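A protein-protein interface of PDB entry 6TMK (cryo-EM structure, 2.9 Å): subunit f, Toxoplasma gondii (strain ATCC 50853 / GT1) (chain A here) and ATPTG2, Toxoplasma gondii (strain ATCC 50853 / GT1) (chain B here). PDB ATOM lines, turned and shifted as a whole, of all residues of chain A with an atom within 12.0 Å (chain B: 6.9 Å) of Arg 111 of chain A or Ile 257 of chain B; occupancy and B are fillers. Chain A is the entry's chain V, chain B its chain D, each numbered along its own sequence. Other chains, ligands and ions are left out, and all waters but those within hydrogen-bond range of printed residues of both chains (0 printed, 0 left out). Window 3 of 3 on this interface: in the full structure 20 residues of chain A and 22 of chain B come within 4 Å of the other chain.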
ATOM      1  N   ASN A 107      -7.696  14.776 -29.342  1.00  0.00           N
ATOM      2  CA  ASN A 107      -7.743  15.853 -28.382  1.00  0.00           C
ATOM      3  C   ASN A 107      -6.433  15.917 -27.611  1.00  0.00           C
ATOM      4  O   ASN A 107      -5.710  14.925 -27.510  1.00  0.00           O
ATOM      5  CB  ASN A 107      -8.902  15.661 -27.417  1.00  0.00           C
ATOM      6  CG  ASN A 107     -10.219  15.503 -28.117  1.00  0.00           C
ATOM      7  OD1 ASN A 107     -10.375  15.875 -29.275  1.00  0.00           O
ATOM      8  ND2 ASN A 107     -11.177  14.931 -27.420  1.00  0.00           N
ATOM      9  N   PRO A 108      -6.104  17.074 -27.051  1.00  0.00           N
ATOM     10  CA  PRO A 108      -4.899  17.173 -26.229  1.00  0.00           C
ATOM     11  C   PRO A 108      -4.981  16.291 -24.997  1.00  0.00           C
ATOM     12  O   PRO A 108      -6.058  15.918 -24.530  1.00  0.00           O
ATOM     13  CB  PRO A 108      -4.850  18.658 -25.855  1.00  0.00           C
ATOM     14  CG  PRO A 108      -6.209  19.152 -26.064  1.00  0.00           C
ATOM     15  CD  PRO A 108      -6.768  18.376 -27.189  1.00  0.00           C
ATOM     16  N   VAL A 109      -3.815  15.951 -24.470  1.00  0.00           N
ATOM     17  CA  VAL A 109      -3.772  15.063 -23.307  1.00  0.00           C
ATOM     18  C   VAL A 109      -4.416  15.774 -22.123  1.00  0.00           C
ATOM     19  O   VAL A 109      -4.081  16.940 -21.850  1.00  0.00           O
ATOM     20  CB  VAL A 109      -2.335  14.665 -22.987  1.00  0.00           C
ATOM     21  CG1 VAL A 109      -2.312  13.729 -21.798  1.00  0.00           C
ATOM     22  CG2 VAL A 109      -1.685  14.019 -24.187  1.00  0.00           C
ATOM     23  N   PRO A 110      -5.334  15.139 -21.400  1.00  0.00           N
ATOM     24  CA  PRO A 110      -5.989  15.837 -20.294  1.00  0.00           C
ATOM     25  C   PRO A 110      -5.014  16.126 -19.168  1.00  0.00           C
ATOM     26  O   PRO A 110      -4.169  15.297 -18.823  1.00  0.00           O
ATOM     27  CB  PRO A 110      -7.077  14.856 -19.844  1.00  0.00           C
ATOM     28  CG  PRO A 110      -7.111  13.778 -20.882  1.00  0.00           C
ATOM     29  CD  PRO A 110      -5.769  13.738 -21.481  1.00  0.00           C
ATOM     30  N   ARG A 111      -5.127  17.322 -18.606  1.00  0.00           N
ATOM     31  CA  ARG A 111      -4.267  17.715 -17.508  1.00  0.00           C
ATOM     32  C   ARG A 111      -4.995  17.486 -16.187  1.00  0.00           C
ATOM     33  O   ARG A 111      -6.201  17.702 -16.090  1.00  0.00           O
ATOM     34  CB  ARG A 111      -3.833  19.174 -17.636  1.00  0.00           C
ATOM     35  CG  ARG A 111      -2.778  19.433 -18.684  1.00  0.00           C
ATOM     36  CD  ARG A 111      -1.932  20.603 -18.258  1.00  0.00           C
ATOM     37  NE  ARG A 111      -0.981  20.219 -17.224  1.00  0.00           N
ATOM     38  CZ  ARG A 111      -0.214  21.071 -16.559  1.00  0.00           C
ATOM     39  NH1 ARG A 111      -0.280  22.367 -16.819  1.00  0.00           N
ATOM     40  NH2 ARG A 111       0.614  20.619 -15.630  1.00  0.00           N
ATOM     41  OXT ARG A 111      -4.399  17.079 -15.191  1.00  0.00           O
ATOM     42  N   GLY B 246      -7.924   9.438 -17.132  1.00  0.00           N
ATOM     43  CA  GLY B 246      -9.232   9.911 -17.517  1.00  0.00           C
ATOM     44  C   GLY B 246      -9.370  11.411 -17.475  1.00  0.00           C
ATOM     45  O   GLY B 246      -8.891  12.063 -16.545  1.00  0.00           O
ATOM     46  N   LYS B 247     -10.037  11.969 -18.482  1.00  0.00           N
ATOM     47  CA  LYS B 247     -10.364  13.385 -18.444  1.00  0.00           C
ATOM     48  C   LYS B 247     -11.334  13.692 -17.312  1.00  0.00           C
ATOM     49  O   LYS B 247     -11.169  14.685 -16.595  1.00  0.00           O
ATOM     50  CB  LYS B 247     -10.954  13.805 -19.786  1.00  0.00           C
ATOM     51  CG  LYS B 247     -10.983  15.293 -20.008  1.00  0.00           C
ATOM     52  CD  LYS B 247     -12.068  15.688 -20.984  1.00  0.00           C
ATOM     53  CE  LYS B 247     -11.703  16.952 -21.740  1.00  0.00           C
ATOM     54  NZ  LYS B 247     -11.107  17.994 -20.859  1.00  0.00           N
ATOM     55  N   THR B 252      -7.703  11.242 -10.678  1.00  0.00           N
ATOM     56  CA  THR B 252      -6.601  12.066 -11.143  1.00  0.00           C
ATOM     57  C   THR B 252      -6.691  13.515 -10.697  1.00  0.00           C
ATOM     58  O   THR B 252      -5.740  14.269 -10.919  1.00  0.00           O
ATOM     59  CB  THR B 252      -6.537  12.031 -12.674  1.00  0.00           C
ATOM     60  OG1 THR B 252      -7.833  12.323 -13.208  1.00  0.00           O
ATOM     61  CG2 THR B 252      -6.104  10.690 -13.164  1.00  0.00           C
ATOM     62  N   LYS B 253      -7.793  13.925 -10.081  1.00  0.00           N
ATOM     63  CA  LYS B 253      -8.040  15.326  -9.769  1.00  0.00           C
ATOM     64  C   LYS B 253      -7.731  15.584  -8.302  1.00  0.00           C
ATOM     65  O   LYS B 253      -8.404  15.050  -7.415  1.00  0.00           O
ATOM     66  CB  LYS B 253      -9.489  15.694 -10.074  1.00  0.00           C
ATOM     67  CG  LYS B 253      -9.959  15.329 -11.454  1.00  0.00           C
ATOM     68  CD  LYS B 253     -11.410  15.703 -11.629  1.00  0.00           C
ATOM     69  CE  LYS B 253     -11.950  15.257 -12.966  1.00  0.00           C
ATOM     70  NZ  LYS B 253     -13.396  14.931 -12.855  1.00  0.00           N
ATOM     71  N   PHE B 255      -6.471  19.223  -7.330  1.00  0.00           N
ATOM     72  CA  PHE B 255      -6.885  20.611  -7.341  1.00  0.00           C
ATOM     73  C   PHE B 255      -7.142  21.028  -8.778  1.00  0.00           C
ATOM     74  O   PHE B 255      -6.501  20.513  -9.698  1.00  0.00           O
ATOM     75  CB  PHE B 255      -5.806  21.509  -6.723  1.00  0.00           C
ATOM     76  CG  PHE B 255      -5.426  21.124  -5.327  1.00  0.00           C
ATOM     77  CD1 PHE B 255      -6.187  21.527  -4.251  1.00  0.00           C
ATOM     78  CD2 PHE B 255      -4.318  20.339  -5.095  1.00  0.00           C
ATOM     79  CE1 PHE B 255      -5.842  21.167  -2.975  1.00  0.00           C
ATOM     80  CE2 PHE B 255      -3.973  19.975  -3.821  1.00  0.00           C
ATOM     81  CZ  PHE B 255      -4.737  20.389  -2.759  1.00  0.00           C
ATOM     82  N   PRO B 256      -8.073  21.949  -9.005  1.00  0.00           N
ATOM     83  CA  PRO B 256      -8.363  22.357 -10.380  1.00  0.00           C
ATOM     84  C   PRO B 256      -7.189  23.081 -11.012  1.00  0.00           C
ATOM     85  O   PRO B 256      -6.511  23.890 -10.374  1.00  0.00           O
ATOM     86  CB  PRO B 256      -9.579  23.273 -10.222  1.00  0.00           C
ATOM     87  CG  PRO B 256      -9.464  23.796  -8.844  1.00  0.00           C
ATOM     88  CD  PRO B 256      -8.903  22.678  -8.036  1.00  0.00           C
ATOM     89  N   ILE B 257      -6.952  22.773 -12.279  1.00  0.00           N
ATOM     90  CA  ILE B 257      -5.883  23.395 -13.052  1.00  0.00           C
ATOM     91  C   ILE B 257      -6.440  24.663 -13.681  1.00  0.00           C
ATOM     92  O   ILE B 257      -7.542  24.636 -14.246  1.00  0.00           O
ATOM     93  CB  ILE B 257      -5.321  22.422 -14.096  1.00  0.00           C
ATOM     94  CG1 ILE B 257      -4.557  21.311 -13.380  1.00  0.00           C
ATOM     95  CG2 ILE B 257      -4.413  23.151 -15.070  1.00  0.00           C
ATOM     96  CD1 ILE B 257      -4.430  20.063 -14.172  1.00  0.00           C
ATOM     97  N   PRO B 258      -5.747  25.794 -13.592  1.00  0.00           N
ATOM     98  CA  PRO B 258      -6.311  27.028 -14.136  1.00  0.00           C
ATOM     99  C   PRO B 258      -6.489  27.021 -15.649  1.00  0.00           C
ATOM    100  O   PRO B 258      -5.793  26.330 -16.412  1.00  0.00           O
ATOM    101  CB  PRO B 258      -5.306  28.098 -13.695  1.00  0.00           C
ATOM    102  CG  PRO B 258      -4.056  27.367 -13.434  1.00  0.00           C
ATOM    103  CD  PRO B 258      -4.473  26.041 -12.903  1.00  0.00           C
ATOM    104  N   ASP B 259      -7.439  27.852 -16.076  1.00  0.00           N
ATOM    105  CA  ASP B 259      -7.846  27.852 -17.468  1.00  0.00           C
ATOM    106  C   ASP B 259      -6.726  28.369 -18.350  1.00  0.00           C
ATOM    107  O   ASP B 259      -6.570  27.912 -19.486  1.00  0.00           O
ATOM    108  CB  ASP B 259      -9.105  28.699 -17.638  1.00  0.00           C
ATOM    109  CG  ASP B 259     -10.378  27.922 -17.348  1.00  0.00           C
ATOM    110  OD1 ASP B 259     -10.298  26.699 -17.107  1.00  0.00           O
ATOM    111  OD2 ASP B 259     -11.464  28.539 -17.351  1.00  0.00           O
ATOM    112  N   HIS B 260      -5.928  29.307 -17.842  1.00  0.00           N
ATOM    113  CA  HIS B 260      -4.837  29.849 -18.629  1.00  0.00           C
ATOM    114  C   HIS B 260      -3.665  28.891 -18.704  1.00  0.00           C
ATOM    115  O   HIS B 260      -2.660  29.209 -19.347  1.00  0.00           O
ATOM    116  CB  HIS B 260      -4.380  31.190 -18.054  1.00  0.00           C
ATOM    117  CG  HIS B 260      -3.801  31.101 -16.678  1.00  0.00           C
ATOM    118  ND1 HIS B 260      -4.565  31.234 -15.539  1.00  0.00           N
ATOM    119  CD2 HIS B 260      -2.530  30.908 -16.259  1.00  0.00           C
ATOM    120  CE1 HIS B 260      -3.788  31.120 -14.477  1.00  0.00           C
ATOM    121  NE2 HIS B 260      -2.550  30.920 -14.886  1.00  0.00           N
ATOM    122  N   GLU B 261      -3.783  27.727 -18.072  1.00  0.00           N
ATOM    123  CA  GLU B 261      -2.780  26.686 -18.160  1.00  0.00           C
ATOM    124  C   GLU B 261      -3.344  25.436 -18.807  1.00  0.00           C
ATOM    125  O   GLU B 261      -2.608  24.460 -18.990  1.00  0.00           O
ATOM    126  CB  GLU B 261      -2.227  26.360 -16.769  1.00  0.00           C
ATOM    127  CG  GLU B 261      -1.238  27.380 -16.241  1.00  0.00           C
ATOM    128  CD  GLU B 261       0.137  27.249 -16.874  1.00  0.00           C
ATOM    129  OE1 GLU B 261       0.682  26.126 -16.882  1.00  0.00           O
ATOM    130  OE2 GLU B 261       0.672  28.264 -17.368  1.00  0.00           O
ATOM    131  N   GLN B 262      -4.631  25.440 -19.162  1.00  0.00           N
ATOM    132  CA  GLN B 262      -5.154  24.270 -19.851  1.00  0.00           C
ATOM    133  C   GLN B 262      -4.993  24.433 -21.363  1.00  0.00           C
ATOM    134  O   GLN B 262      -5.093  25.546 -21.885  1.00  0.00           O
ATOM    135  CB  GLN B 262      -6.622  24.053 -19.508  1.00  0.00           C
ATOM    136  CG  GLN B 262      -6.850  23.662 -18.075  1.00  0.00           C
ATOM    137  CD  GLN B 262      -8.088  22.833 -17.900  1.00  0.00           C
ATOM    138  OE1 GLN B 262      -9.188  23.358 -17.735  1.00  0.00           O
ATOM    139  NE2 GLN B 262      -7.925  21.522 -17.963  1.00  0.00           N
ATOM    140  N   PRO B 263      -4.741  23.361 -22.109  1.00  0.00           N
ATOM    141  CA  PRO B 263      -4.506  23.494 -23.547  1.00  0.00           C
ATOM    142  C   PRO B 263      -5.781  23.502 -24.380  1.00  0.00           C
ATOM    143  O   PRO B 263      -6.835  23.015 -23.973  1.00  0.00           O
ATOM    144  CB  PRO B 263      -3.657  22.257 -23.859  1.00  0.00           C
ATOM    145  CG  PRO B 263      -4.146  21.256 -22.936  1.00  0.00           C
ATOM    146  CD  PRO B 263      -4.535  21.972 -21.667  1.00  0.00           C
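Of chain B, only Ile 257 (3.2 Å) and Glu 261 (3.8 Å) come within 4 Å of Arg 111 of chain A.
Of chain A, only Arg 111 (3.2 Å) comes within 4 Å of Ile 257 of chain B.
No residue of chain A comes within 4 Å of Pro 258 of chain B.
No residue of chain A comes within 4 Å of Asp 259 of chain B.
Glu 261 of chain B touches just one residue of chain A: Arg 111.
Of the printed residues of chain B, Pro 108 of chain A touches Pro 263 (3.97 Å).
Printed residues of chain B within 4 Å of Pro 110 of chain A: Lys 247 (3.9 Å).
The nearest residue of chain A that does not touch Ile 257 of chain B is Pro 110 of chain A (6.4 Å).
The nearest printed residue of chain B that does not touch Pro 110 of chain A is Gly 246 of chain B (4.7 Å).
Pro 108 of chain A touches Pro 263 of chain B.
CB of Pro 110 of chain A touches CA of Lys 247 of chain B (3.9 Å).
Ile 257 of chain B touches Arg 111 of chain A (CD1 to OXT, 3.2 Å).
The side-chain carboxylate (OE1) of Glu 261 of chain B lies within salt-bridge range of the guanidinium group (NH1) of Arg 111 of chain A (3.9 Å).
Of the 13 printed residues of chain B, 4 touch a printed residue of chain A.
Hydrophobic or aromatic side chains of chain B that line the printed part of chain A: Ile 257 and Pro 263.
Along chain B the printed residues that touch a printed residue of chain A span positions 247 to 263.
Hydrophobic or aromatic side chains of chain A within 4 Å of the printed part of chain B: Pro 108 and Pro 110.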
